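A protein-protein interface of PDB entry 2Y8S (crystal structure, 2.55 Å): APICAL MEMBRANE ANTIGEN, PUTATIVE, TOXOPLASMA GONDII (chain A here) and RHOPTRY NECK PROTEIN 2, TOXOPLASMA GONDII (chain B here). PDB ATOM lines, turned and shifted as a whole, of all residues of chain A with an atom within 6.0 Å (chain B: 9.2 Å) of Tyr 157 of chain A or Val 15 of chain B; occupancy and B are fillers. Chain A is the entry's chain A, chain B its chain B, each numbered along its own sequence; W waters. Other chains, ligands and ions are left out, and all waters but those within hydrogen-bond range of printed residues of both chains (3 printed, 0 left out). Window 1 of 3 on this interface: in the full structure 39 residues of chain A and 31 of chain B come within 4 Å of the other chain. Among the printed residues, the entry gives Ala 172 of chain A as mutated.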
ATOM      1  N   VAL A  47     -17.295  31.251  39.116  1.00  0.00           N
ATOM      2  CA  VAL A  47     -15.954  30.672  39.127  1.00  0.00           C
ATOM      3  C   VAL A  47     -15.133  31.752  39.778  1.00  0.00           C
ATOM      4  O   VAL A  47     -15.064  32.846  39.230  1.00  0.00           O
ATOM      5  CB  VAL A  47     -15.393  30.448  37.690  1.00  0.00           C
ATOM      6  CG1 VAL A  47     -13.975  29.867  37.730  1.00  0.00           C
ATOM      7  CG2 VAL A  47     -16.289  29.558  36.873  1.00  0.00           C
ATOM      8  N   ASP A  48     -14.544  31.470  40.938  1.00  0.00           N
ATOM      9  CA  ASP A  48     -13.705  32.451  41.675  1.00  0.00           C
ATOM     10  C   ASP A  48     -14.488  33.732  42.052  1.00  0.00           C
ATOM     11  O   ASP A  48     -13.977  34.830  41.949  1.00  0.00           O
ATOM     12  CB  ASP A  48     -12.441  32.787  40.876  1.00  0.00           C
ATOM     13  CG  ASP A  48     -11.636  31.523  40.466  1.00  0.00           C
ATOM     14  OD1 ASP A  48     -11.294  30.700  41.353  1.00  0.00           O
ATOM     15  OD2 ASP A  48     -11.315  31.356  39.255  1.00  0.00           O
ATOM     16  N   GLU A  54     -23.286  31.141  30.623  1.00  0.00           N
ATOM     17  CA  GLU A  54     -23.016  29.810  30.160  1.00  0.00           C
ATOM     18  C   GLU A  54     -24.079  29.356  29.133  1.00  0.00           C
ATOM     19  O   GLU A  54     -25.272  29.512  29.397  1.00  0.00           O
ATOM     20  CB  GLU A  54     -22.983  28.895  31.393  1.00  0.00           C
ATOM     21  CG  GLU A  54     -22.379  27.558  31.179  1.00  0.00           C
ATOM     22  CD  GLU A  54     -22.860  26.593  32.220  1.00  0.00           C
ATOM     23  OE1 GLU A  54     -23.940  26.842  32.816  1.00  0.00           O
ATOM     24  OE2 GLU A  54     -22.173  25.569  32.433  1.00  0.00           O
ATOM     25  N   PRO A  55     -23.653  28.790  27.979  1.00  0.00           N
ATOM     26  CA  PRO A  55     -24.676  28.254  27.038  1.00  0.00           C
ATOM     27  C   PRO A  55     -25.423  27.158  27.776  1.00  0.00           C
ATOM     28  O   PRO A  55     -24.818  26.485  28.634  1.00  0.00           O
ATOM     29  CB  PRO A  55     -23.835  27.674  25.895  1.00  0.00           C
ATOM     30  CG  PRO A  55     -22.537  28.476  25.951  1.00  0.00           C
ATOM     31  CD  PRO A  55     -22.289  28.626  27.442  1.00  0.00           C
ATOM     32  N   LEU A 103     -10.792  23.959  22.537  1.00  0.00           N
ATOM     33  CA  LEU A 103     -10.030  23.764  23.760  1.00  0.00           C
ATOM     34  C   LEU A 103      -8.795  22.851  23.522  1.00  0.00           C
ATOM     35  O   LEU A 103      -8.916  21.736  23.014  1.00  0.00           O
ATOM     36  CB  LEU A 103     -10.956  23.233  24.840  1.00  0.00           C
ATOM     37  CG  LEU A 103     -10.373  23.032  26.241  1.00  0.00           C
ATOM     38  CD1 LEU A 103     -10.001  24.379  26.921  1.00  0.00           C
ATOM     39  CD2 LEU A 103     -11.340  22.194  27.080  1.00  0.00           C
ATOM     40  N   PHE A 105      -6.365  21.726  25.792  1.00  0.00           N
ATOM     41  CA  PHE A 105      -5.825  21.101  26.981  1.00  0.00           C
ATOM     42  C   PHE A 105      -5.453  19.621  26.800  1.00  0.00           C
ATOM     43  O   PHE A 105      -6.086  18.885  26.043  1.00  0.00           O
ATOM     44  CB  PHE A 105      -6.837  21.229  28.113  1.00  0.00           C
ATOM     45  CG  PHE A 105      -7.056  22.636  28.593  1.00  0.00           C
ATOM     46  CD1 PHE A 105      -6.460  23.729  27.951  1.00  0.00           C
ATOM     47  CD2 PHE A 105      -7.925  22.880  29.673  1.00  0.00           C
ATOM     48  CE1 PHE A 105      -6.681  25.058  28.412  1.00  0.00           C
ATOM     49  CE2 PHE A 105      -8.173  24.198  30.133  1.00  0.00           C
ATOM     50  CZ  PHE A 105      -7.548  25.303  29.508  1.00  0.00           C
ATOM     51  N   ALA A 140     -19.202  16.302  26.721  1.00  0.00           N
ATOM     52  CA  ALA A 140     -19.167  17.725  27.023  1.00  0.00           C
ATOM     53  C   ALA A 140     -19.730  17.962  28.401  1.00  0.00           C
ATOM     54  O   ALA A 140     -19.172  18.721  29.203  1.00  0.00           O
ATOM     55  CB  ALA A 140     -19.968  18.542  25.960  1.00  0.00           C
ATOM     56  N   THR A 143     -17.407  17.486  31.472  1.00  0.00           N
ATOM     57  CA  THR A 143     -16.257  18.334  31.484  1.00  0.00           C
ATOM     58  C   THR A 143     -16.635  19.615  32.214  1.00  0.00           C
ATOM     59  O   THR A 143     -17.543  20.360  31.760  1.00  0.00           O
ATOM     60  CB  THR A 143     -15.884  18.694  30.052  1.00  0.00           C
ATOM     61  OG1 THR A 143     -15.894  17.507  29.241  1.00  0.00           O
ATOM     62  CG2 THR A 143     -14.499  19.363  30.005  1.00  0.00           C
ATOM     63  N   VAL A 144     -15.992  19.889  33.344  1.00  0.00           N
ATOM     64  CA  VAL A 144     -16.290  21.152  34.016  1.00  0.00           C
ATOM     65  C   VAL A 144     -15.009  21.920  34.180  1.00  0.00           C
ATOM     66  O   VAL A 144     -13.949  21.322  34.208  1.00  0.00           O
ATOM     67  CB  VAL A 144     -17.040  20.943  35.400  1.00  0.00           C
ATOM     68  CG1 VAL A 144     -18.193  19.892  35.272  1.00  0.00           C
ATOM     69  CG2 VAL A 144     -16.073  20.535  36.484  1.00  0.00           C
ATOM     70  N   ALA A 145     -15.086  23.237  34.270  1.00  0.00           N
ATOM     71  CA  ALA A 145     -13.882  24.041  34.523  1.00  0.00           C
ATOM     72  C   ALA A 145     -13.443  23.926  35.951  1.00  0.00           C
ATOM     73  O   ALA A 145     -14.248  23.765  36.839  1.00  0.00           O
ATOM     74  CB  ALA A 145     -14.103  25.527  34.183  1.00  0.00           C
ATOM     75  N   MET A 146     -12.145  24.078  36.147  1.00  0.00           N
ATOM     76  CA  MET A 146     -11.542  24.136  37.465  1.00  0.00           C
ATOM     77  C   MET A 146     -11.160  25.562  37.826  1.00  0.00           C
ATOM     78  O   MET A 146     -10.600  26.299  36.997  1.00  0.00           O
ATOM     79  CB  MET A 146     -10.324  23.236  37.471  1.00  0.00           C
ATOM     80  CG  MET A 146     -10.696  21.810  37.138  1.00  0.00           C
ATOM     81  SD  MET A 146      -9.301  20.730  36.830  1.00  0.00           S
ATOM     82  CE  MET A 146      -8.293  21.035  38.307  1.00  0.00           C
ATOM     83  N   ASP A 147     -11.441  25.949  39.065  1.00  0.00           N
ATOM     84  CA  ASP A 147     -11.175  27.323  39.514  1.00  0.00           C
ATOM     85  C   ASP A 147      -9.723  27.570  39.933  1.00  0.00           C
ATOM     86  O   ASP A 147      -8.871  26.693  39.809  1.00  0.00           O
ATOM     87  CB  ASP A 147     -12.120  27.688  40.656  1.00  0.00           C
ATOM     88  CG  ASP A 147     -11.868  26.867  41.895  1.00  0.00           C
ATOM     89  OD1 ASP A 147     -10.837  26.147  41.956  1.00  0.00           O
ATOM     90  OD2 ASP A 147     -12.707  26.950  42.815  1.00  0.00           O
ATOM     91  N   TYR A 155     -19.286  25.066  35.870  1.00  0.00           N
ATOM     92  CA  TYR A 155     -19.244  25.714  34.533  1.00  0.00           C
ATOM     93  C   TYR A 155     -18.816  24.781  33.405  1.00  0.00           C
ATOM     94  O   TYR A 155     -17.758  24.172  33.475  1.00  0.00           O
ATOM     95  CB  TYR A 155     -18.317  26.937  34.542  1.00  0.00           C
ATOM     96  CG  TYR A 155     -18.270  27.723  33.241  1.00  0.00           C
ATOM     97  CD1 TYR A 155     -17.437  27.333  32.199  1.00  0.00           C
ATOM     98  CD2 TYR A 155     -19.056  28.864  33.061  1.00  0.00           C
ATOM     99  CE1 TYR A 155     -17.398  28.052  30.972  1.00  0.00           C
ATOM    100  CE2 TYR A 155     -19.007  29.614  31.861  1.00  0.00           C
ATOM    101  CZ  TYR A 155     -18.172  29.205  30.831  1.00  0.00           C
ATOM    102  OH  TYR A 155     -18.140  29.956  29.689  1.00  0.00           O
ATOM    103  N   ARG A 156     -19.619  24.713  32.350  1.00  0.00           N
ATOM    104  CA  ARG A 156     -19.361  23.799  31.232  1.00  0.00           C
ATOM    105  C   ARG A 156     -19.302  24.545  29.881  1.00  0.00           C
ATOM    106  O   ARG A 156     -20.151  25.434  29.581  1.00  0.00           O
ATOM    107  CB  ARG A 156     -20.459  22.747  31.184  1.00  0.00           C
ATOM    108  CG  ARG A 156     -20.536  21.880  32.431  1.00  0.00           C
ATOM    109  CD  ARG A 156     -21.584  20.778  32.313  1.00  0.00           C
ATOM    110  NE  ARG A 156     -21.491  19.804  33.410  1.00  0.00           N
ATOM    111  CZ  ARG A 156     -21.928  20.021  34.657  1.00  0.00           C
ATOM    112  NH1 ARG A 156     -22.486  21.185  35.002  1.00  0.00           N
ATOM    113  NH2 ARG A 156     -21.816  19.071  35.574  1.00  0.00           N
ATOM    114  N   TYR A 157     -18.298  24.202  29.076  1.00  0.00           N
ATOM    115  CA  TYR A 157     -18.105  24.783  27.766  1.00  0.00           C
ATOM    116  C   TYR A 157     -18.940  24.050  26.720  1.00  0.00           C
ATOM    117  O   TYR A 157     -19.194  22.874  26.887  1.00  0.00           O
ATOM    118  CB  TYR A 157     -16.665  24.676  27.390  1.00  0.00           C
ATOM    119  CG  TYR A 157     -15.746  25.457  28.296  1.00  0.00           C
ATOM    120  CD1 TYR A 157     -15.483  26.814  28.065  1.00  0.00           C
ATOM    121  CD2 TYR A 157     -15.154  24.851  29.398  1.00  0.00           C
ATOM    122  CE1 TYR A 157     -14.645  27.518  28.860  1.00  0.00           C
ATOM    123  CE2 TYR A 157     -14.288  25.562  30.218  1.00  0.00           C
ATOM    124  CZ  TYR A 157     -14.029  26.892  29.947  1.00  0.00           C
ATOM    125  OH  TYR A 157     -13.173  27.610  30.794  1.00  0.00           O
ATOM    126  N   PRO A 158     -19.398  24.766  25.654  1.00  0.00           N
ATOM    127  CA  PRO A 158     -20.210  24.112  24.676  1.00  0.00           C
ATOM    128  C   PRO A 158     -19.344  23.230  23.768  1.00  0.00           C
ATOM    129  O   PRO A 158     -18.091  23.286  23.854  1.00  0.00           O
ATOM    130  CB  PRO A 158     -20.811  25.280  23.901  1.00  0.00           C
ATOM    131  CG  PRO A 158     -19.834  26.349  23.999  1.00  0.00           C
ATOM    132  CD  PRO A 158     -19.259  26.209  25.374  1.00  0.00           C
ATOM    133  N   PHE A 159     -20.004  22.444  22.920  1.00  0.00           N
ATOM    134  CA  PHE A 159     -19.339  21.495  22.066  1.00  0.00           C
ATOM    135  C   PHE A 159     -19.815  21.657  20.624  1.00  0.00           C
ATOM    136  O   PHE A 159     -20.869  22.231  20.362  1.00  0.00           O
ATOM    137  CB  PHE A 159     -19.635  20.050  22.509  1.00  0.00           C
ATOM    138  CG  PHE A 159     -21.047  19.598  22.186  1.00  0.00           C
ATOM    139  CD1 PHE A 159     -21.339  19.005  20.963  1.00  0.00           C
ATOM    140  CD2 PHE A 159     -22.093  19.784  23.105  1.00  0.00           C
ATOM    141  CE1 PHE A 159     -22.648  18.603  20.659  1.00  0.00           C
ATOM    142  CE2 PHE A 159     -23.372  19.371  22.819  1.00  0.00           C
ATOM    143  CZ  PHE A 159     -23.656  18.769  21.579  1.00  0.00           C
ATOM    144  N   ILE A 170     -14.708  20.400  22.270  1.00  0.00           N
ATOM    145  CA  ILE A 170     -15.163  21.202  23.373  1.00  0.00           C
ATOM    146  C   ILE A 170     -14.601  22.564  23.063  1.00  0.00           C
ATOM    147  O   ILE A 170     -13.421  22.662  22.759  1.00  0.00           O
ATOM    148  CB  ILE A 170     -14.626  20.690  24.760  1.00  0.00           C
ATOM    149  CG1 ILE A 170     -14.921  19.190  24.971  1.00  0.00           C
ATOM    150  CG2 ILE A 170     -15.238  21.494  25.951  1.00  0.00           C
ATOM    151  CD1 ILE A 170     -16.425  18.856  24.912  1.00  0.00           C
ATOM    152  N   LEU A 171     -15.422  23.610  23.116  1.00  0.00           N
ATOM    153  CA  LEU A 171     -14.932  24.936  22.745  1.00  0.00           C
ATOM    154  C   LEU A 171     -14.463  25.720  23.959  1.00  0.00           C
ATOM    155  O   LEU A 171     -15.168  25.787  24.944  1.00  0.00           O
ATOM    156  CB  LEU A 171     -16.005  25.748  22.026  1.00  0.00           C
ATOM    157  CG  LEU A 171     -16.549  25.094  20.759  1.00  0.00           C
ATOM    158  CD1 LEU A 171     -17.562  25.973  20.056  1.00  0.00           C
ATOM    159  CD2 LEU A 171     -15.405  24.664  19.817  1.00  0.00           C
ATOM    160  N   ALA A 172     -13.286  26.332  23.894  1.00  0.00           N
ATOM    161  CA  ALA A 172     -12.780  27.056  25.049  1.00  0.00           C
ATOM    162  C   ALA A 172     -13.440  28.406  25.086  1.00  0.00           C
ATOM    163  O   ALA A 172     -13.159  29.187  25.975  1.00  0.00           O
ATOM    164  CB  ALA A 172     -11.261  27.210  24.980  1.00  0.00           C
ATOM    165  N   VAL A 173     -14.301  28.677  24.109  1.00  0.00           N
ATOM    166  CA  VAL A 173     -14.886  30.002  23.905  1.00  0.00           C
ATOM    167  C   VAL A 173     -16.408  29.838  23.781  1.00  0.00           C
ATOM    168  O   VAL A 173     -16.912  29.116  22.899  1.00  0.00           O
ATOM    169  CB  VAL A 173     -14.269  30.684  22.652  1.00  0.00           C
ATOM    170  CG1 VAL A 173     -15.020  31.966  22.275  1.00  0.00           C
ATOM    171  CG2 VAL A 173     -12.809  31.008  22.880  1.00  0.00           C
ATOM    172  N   SER A 174     -17.122  30.480  24.705  1.00  0.00           N
ATOM    173  CA  SER A 174     -18.577  30.410  24.779  1.00  0.00           C
ATOM    174  C   SER A 174     -19.265  31.570  24.082  1.00  0.00           C
ATOM    175  O   SER A 174     -20.435  31.430  23.677  1.00  0.00           O
ATOM    176  CB  SER A 174     -19.045  30.340  26.230  1.00  0.00           C
ATOM    177  OG  SER A 174     -18.072  29.645  26.991  1.00  0.00           O
ATOM    178  N   GLY A 213     -23.710  22.770  20.348  1.00  0.00           N
ATOM    179  CA  GLY A 213     -24.645  22.549  21.442  1.00  0.00           C
ATOM    180  C   GLY A 213     -24.064  23.064  22.716  1.00  0.00           C
ATOM    181  O   GLY A 213     -22.835  23.164  22.824  1.00  0.00           O
ATOM    182  N   SER A 214     -24.921  23.385  23.687  1.00  0.00           N
ATOM    183  CA  SER A 214     -24.440  23.674  25.054  1.00  0.00           C
ATOM    184  C   SER A 214     -24.104  22.317  25.649  1.00  0.00           C
ATOM    185  O   SER A 214     -24.569  21.297  25.126  1.00  0.00           O
ATOM    186  CB  SER A 214     -25.504  24.409  25.910  1.00  0.00           C
ATOM    187  OG  SER A 214     -26.420  23.523  26.545  1.00  0.00           O
ATOM    188  N   ALA A 215     -23.318  22.282  26.730  1.00  0.00           N
ATOM    189  CA  ALA A 215     -22.939  20.982  27.301  1.00  0.00           C
ATOM    190  C   ALA A 215     -24.135  20.314  27.964  1.00  0.00           C
ATOM    191  O   ALA A 215     -24.046  19.167  28.413  1.00  0.00           O
ATOM    192  CB  ALA A 215     -21.791  21.105  28.269  1.00  0.00           C
ATOM    193  N   GLY B  10     -20.641  36.644  26.896  1.00  0.00           N
ATOM    194  CA  GLY B  10     -20.225  35.256  27.161  1.00  0.00           C
ATOM    195  C   GLY B  10     -18.733  34.969  27.330  1.00  0.00           C
ATOM    196  O   GLY B  10     -18.324  33.840  27.276  1.00  0.00           O
ATOM    197  N   GLY B  11     -17.927  36.007  27.538  1.00  0.00           N
ATOM    198  CA  GLY B  11     -16.514  35.882  27.854  1.00  0.00           C
ATOM    199  C   GLY B  11     -16.303  34.874  28.942  1.00  0.00           C
ATOM    200  O   GLY B  11     -17.061  34.828  29.914  1.00  0.00           O
ATOM    201  N   ALA B  12     -15.273  34.044  28.781  1.00  0.00           N
ATOM    202  CA  ALA B  12     -15.163  32.850  29.615  1.00  0.00           C
ATOM    203  C   ALA B  12     -14.358  33.043  30.915  1.00  0.00           C
ATOM    204  O   ALA B  12     -13.561  33.986  31.045  1.00  0.00           O
ATOM    205  CB  ALA B  12     -14.591  31.748  28.787  1.00  0.00           C
ATOM    206  N   PRO B  13     -14.546  32.143  31.896  1.00  0.00           N
ATOM    207  CA  PRO B  13     -13.665  32.315  33.051  1.00  0.00           C
ATOM    208  C   PRO B  13     -12.232  32.048  32.613  1.00  0.00           C
ATOM    209  O   PRO B  13     -12.006  31.222  31.736  1.00  0.00           O
ATOM    210  CB  PRO B  13     -14.164  31.278  34.052  1.00  0.00           C
ATOM    211  CG  PRO B  13     -15.060  30.355  33.291  1.00  0.00           C
ATOM    212  CD  PRO B  13     -15.406  30.939  31.986  1.00  0.00           C
ATOM    213  N   PRO B  14     -11.271  32.785  33.178  1.00  0.00           N
ATOM    214  CA  PRO B  14      -9.855  32.573  32.817  1.00  0.00           C
ATOM    215  C   PRO B  14      -9.259  31.348  33.561  1.00  0.00           C
ATOM    216  O   PRO B  14      -8.836  31.456  34.713  1.00  0.00           O
ATOM    217  CB  PRO B  14      -9.179  33.881  33.263  1.00  0.00           C
ATOM    218  CG  PRO B  14     -10.060  34.361  34.460  1.00  0.00           C
ATOM    219  CD  PRO B  14     -11.463  33.867  34.175  1.00  0.00           C
ATOM    220  N   VAL B  15      -9.186  30.224  32.865  1.00  0.00           N
ATOM    221  CA  VAL B  15      -9.064  28.899  33.454  1.00  0.00           C
ATOM    222  C   VAL B  15      -7.947  28.158  32.732  1.00  0.00           C
ATOM    223  O   VAL B  15      -7.695  28.408  31.556  1.00  0.00           O
ATOM    224  CB  VAL B  15     -10.452  28.194  33.279  1.00  0.00           C
ATOM    225  CG1 VAL B  15     -10.351  26.728  32.871  1.00  0.00           C
ATOM    226  CG2 VAL B  15     -11.279  28.390  34.512  1.00  0.00           C
ATOM    227  N   SER B  16      -7.269  27.248  33.420  1.00  0.00           N
ATOM    228  CA  SER B  16      -6.105  26.567  32.816  1.00  0.00           C
ATOM    229  C   SER B  16      -6.293  25.067  32.732  1.00  0.00           C
ATOM    230  O   SER B  16      -5.558  24.372  32.002  1.00  0.00           O
ATOM    231  CB  SER B  16      -4.851  26.860  33.631  1.00  0.00           C
ATOM    232  OG  SER B  16      -4.371  28.169  33.351  1.00  0.00           O
ATOM    233  N   CYS B  17      -7.261  24.578  33.501  1.00  0.00           N
ATOM    234  CA  CYS B  17      -7.554  23.156  33.582  1.00  0.00           C
ATOM    235  C   CYS B  17      -9.032  22.935  33.562  1.00  0.00           C
ATOM    236  O   CYS B  17      -9.794  23.786  33.939  1.00  0.00           O
ATOM    237  CB  CYS B  17      -6.954  22.507  34.848  1.00  0.00           C
ATOM    238  SG  CYS B  17      -5.185  22.714  34.944  1.00  0.00           S
ATOM    239  N   VAL B  18      -9.418  21.753  33.149  1.00  0.00           N
ATOM    240  CA  VAL B  18     -10.790  21.323  33.153  1.00  0.00           C
ATOM    241  C   VAL B  18     -10.738  19.884  33.711  1.00  0.00           C
ATOM    242  O   VAL B  18      -9.724  19.200  33.486  1.00  0.00           O
ATOM    243  CB  VAL B  18     -11.257  21.328  31.704  1.00  0.00           C
ATOM    244  CG1 VAL B  18     -12.285  20.330  31.506  1.00  0.00           C
ATOM    245  CG2 VAL B  18     -11.738  22.708  31.314  1.00  0.00           C
ATOM    246  N   THR B  19     -11.754  19.419  34.452  1.00  0.00           N
ATOM    247  CA  THR B  19     -11.843  17.960  34.701  1.00  0.00           C
ATOM    248  C   THR B  19     -12.837  17.286  33.816  1.00  0.00           C
ATOM    249  O   THR B  19     -14.008  17.670  33.778  1.00  0.00           O
ATOM    250  CB  THR B  19     -12.273  17.463  36.129  1.00  0.00           C
ATOM    251  OG1 THR B  19     -12.925  18.479  36.915  1.00  0.00           O
ATOM    252  CG2 THR B  19     -11.138  16.872  36.822  1.00  0.00           C
ATOM    253  N   THR B  26      -7.271  17.994  32.944  1.00  0.00           N
ATOM    254  CA  THR B  26      -6.824  18.329  31.625  1.00  0.00           C
ATOM    255  C   THR B  26      -6.345  19.793  31.663  1.00  0.00           C
ATOM    256  O   THR B  26      -7.084  20.669  32.068  1.00  0.00           O
ATOM    257  CB  THR B  26      -8.018  18.034  30.663  1.00  0.00           C
ATOM    258  OG1 THR B  26      -7.590  17.192  29.600  1.00  0.00           O
ATOM    259  CG2 THR B  26      -8.658  19.243  30.157  1.00  0.00           C
ATOM    260  N   CYS B  27      -5.105  20.043  31.270  1.00  0.00           N
ATOM    261  CA  CYS B  27      -4.515  21.390  31.402  1.00  0.00           C
ATOM    262  C   CYS B  27      -3.803  21.865  30.156  1.00  0.00           C
ATOM    263  O   CYS B  27      -3.346  21.068  29.342  1.00  0.00           O
ATOM    264  CB  CYS B  27      -3.550  21.507  32.603  1.00  0.00           C
ATOM    265  SG  CYS B  27      -4.312  21.032  34.141  1.00  0.00           S
ATOM    266  N   ALA B  28      -3.684  23.181  30.048  1.00  0.00           N
ATOM    267  CA  ALA B  28      -2.930  23.791  28.974  1.00  0.00           C
ATOM    268  C   ALA B  28      -1.415  23.513  29.052  1.00  0.00           C
ATOM    269  O   ALA B  28      -0.756  23.902  30.020  1.00  0.00           O
ATOM    270  CB  ALA B  28      -3.224  25.274  28.931  1.00  0.00           C
ATOM    271  N   GLN B  30       0.924  24.859  27.372  1.00  0.00           N
ATOM    272  CA  GLN B  30       1.695  26.103  27.267  1.00  0.00           C
ATOM    273  C   GLN B  30       0.818  27.241  27.704  1.00  0.00           C
ATOM    274  O   GLN B  30      -0.393  27.109  27.695  1.00  0.00           O
ATOM    275  CB  GLN B  30       2.114  26.387  25.836  1.00  0.00           C
ATOM    276  CG  GLN B  30       2.692  25.232  25.076  1.00  0.00           C
ATOM    277  CD  GLN B  30       2.936  25.604  23.621  1.00  0.00           C
ATOM    278  OE1 GLN B  30       3.707  26.534  23.329  1.00  0.00           O
ATOM    279  NE2 GLN B  30       2.277  24.894  22.698  1.00  0.00           N
ATOM    280  N   ALA B  31       1.422  28.361  28.086  1.00  0.00           N
ATOM    281  CA  ALA B  31       0.662  29.542  28.482  1.00  0.00           C
ATOM    282  C   ALA B  31      -0.381  29.935  27.431  1.00  0.00           C
ATOM    283  O   ALA B  31      -0.081  29.981  26.242  1.00  0.00           O
ATOM    284  CB  ALA B  31       1.620  30.716  28.750  1.00  0.00           C
ATOM    285  N   ILE B  32      -1.602  30.214  27.868  1.00  0.00           N
ATOM    286  CA  ILE B  32      -2.648  30.653  26.950  1.00  0.00           C
ATOM    287  C   ILE B  32      -2.512  32.137  26.693  1.00  0.00           C
ATOM    288  O   ILE B  32      -2.254  32.895  27.622  1.00  0.00           O
ATOM    289  CB  ILE B  32      -4.068  30.320  27.504  1.00  0.00           C
ATOM    290  CG1 ILE B  32      -4.381  28.830  27.338  1.00  0.00           C
ATOM    291  CG2 ILE B  32      -5.189  31.142  26.790  1.00  0.00           C
ATOM    292  CD1 ILE B  32      -4.703  28.393  25.872  1.00  0.00           C
ATOM    293  N   ALA B  33      -2.675  32.548  25.441  1.00  0.00           N
ATOM    294  CA  ALA B  33      -2.613  33.962  25.047  1.00  0.00           C
ATOM    295  C   ALA B  33      -3.561  34.874  25.849  1.00  0.00           C
ATOM    296  O   ALA B  33      -4.731  34.521  26.064  1.00  0.00           O
ATOM    297  CB  ALA B  33      -2.866  34.096  23.543  1.00  0.00           C
HETATM  298  O   HOH W   1     -16.134  32.749  25.967  1.00  0.00           O
HETATM  299  O   HOH W   2     -11.733  29.412  29.136  1.00  0.00           O
HETATM  300  O   HOH W   3     -18.742  32.328  29.576  1.00  0.00           O
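The side-chain sulfur (SD) of Met 146 of chain A sits close to the backbone carbonyl oxygen (O) of Val 18 of chain B. N of Thr 19 of chain B sits at hydrogen-bond distance from SD of Met 146 of chain A, at 3.7 Å. The backbone carbonyl oxygen of Cys 17 of chain B is in hydrogen-bond range of the backbone NH of Met 146 of chain A, 3.2 Å away. The backbone carbonyl oxygen (O) of Val 144 of chain A is in hydrogen-bond range of the backbone NH (N) of Thr 19 of chain B.
The side-chain sulfur (SG) of Cys 17 of chain B is disulfide-bonded to the side-chain sulfur (SG) of Cys 27 of chain B (2.1 Å). O of Val 18 of chain B sits at hydrogen-bond distance from N of Thr 26 of chain B, 2.8 Å away. The side-chain hydroxyl of Thr 143 of chain A sits close to the backbone carbonyl oxygen of Ala 140 of chain A, 3.5 Å away. The side-chain hydroxyl (OH) of Tyr 155 of chain A is in hydrogen-bond range of the side-chain hydroxyl (OG) of Ser 174 of chain A (2.7 Å). The backbone NH of Ala 145 of chain A sits at hydrogen-bond distance from the backbone carbonyl oxygen of Tyr 155 of chain A (2.9 Å). The backbone carbonyl oxygen (O) of Ser 16 of chain B is in hydrogen-bond range of the backbone NH (N) of Ala 28 of chain B, 3.0 Å away.
O of Val 15 of chain B touches CZ of Phe 105 of chain A (3.7 Å). Phe 105 of chain A touches Val 18 of chain B. Ala 28 of chain B touches Phe 105 of chain A. Thr 143 of chain A touches Val 18 of chain B (CG2 to CG1, 2.8 Å). Thr 143 of chain A touches Thr 19 of chain B. Val 18 of chain B touches Val 144 of chain A (CG1 to O, 3.3 Å). Pro 13 of chain B touches Tyr 155 of chain A. O of Pro 13 of chain B touches OH of Tyr 157 of chain A, 3.9 Å away. CG1 of Val 15 of chain B touches OH of Tyr 157 of chain A, at 3.6 Å. Gly 10 of chain B touches Ser 174 of chain A.
Glu 54 of chain A touches none of the printed residues of chain B. Printed residues of chain B within 4 Å of Tyr 157 of chain A: Pro 13, Val 15 and Val 18. Of the printed residues of chain A, Val 15 of chain B touches Phe 105, Met 146 and Tyr 157. Of the printed residues of chain A, Ser 16 of chain B touches Phe 105 (3.2 Å). Of the printed residues of chain A, Val 18 of chain B touches Phe 105, Thr 143, Val 144, Met 146 and Tyr 157. Of the printed residues of chain A, Thr 26 of chain B touches Phe 105 (3.4 Å). Gln 30 of chain B touches none of the printed residues of chain A. The nearest printed residue of chain B that does not touch Tyr 157 of chain A is Ala 12 of chain B (4.2 Å). The nearest residue of chain A that does not touch Val 15 of chain B is Ala 145 of chain A (4.03 Å). The nearest printed residue of chain A that does not touch Pro 13 of chain B is Ala 145 of chain A (5.0 Å).
Hydrophobic or aromatic side chains of chain B within 4 Å of the printed part of chain A: Pro 13, Val 15, Val 18 and Ala 28. Along chain A the printed residues that touch a printed residue of chain B span positions 47 to 174. Among the printed residues, 21 pairs touch across the chains. Among the printed residues, no Asp or Glu carboxylate lies within 4 Å of a Lys or Arg side-chain nitrogen of the other chain.
Water W3 lies within hydrogen-bond range of the side-chain hydroxyl (OH) of Tyr 155 of chain A (2.4 Å), the backbone carbonyl oxygen (O) of Gly 10 of chain B (2.8 Å) and the backbone carbonyl oxygen (O) of Gly 11 of chain B (3.0 Å). Water W1 lies within hydrogen-bond range of O of Gly 10 of chain B (2.8 Å), N of Ser 174 of chain A (2.8 Å) and N of Ala 12 of chain B (3.2 Å). Water W2 lies within hydrogen-bond range of OH of Tyr 157 of chain A (2.8 Å), O of Pro 13 of chain B (3.2 Å) and O of Ala 172 of chain A (3.5 Å).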
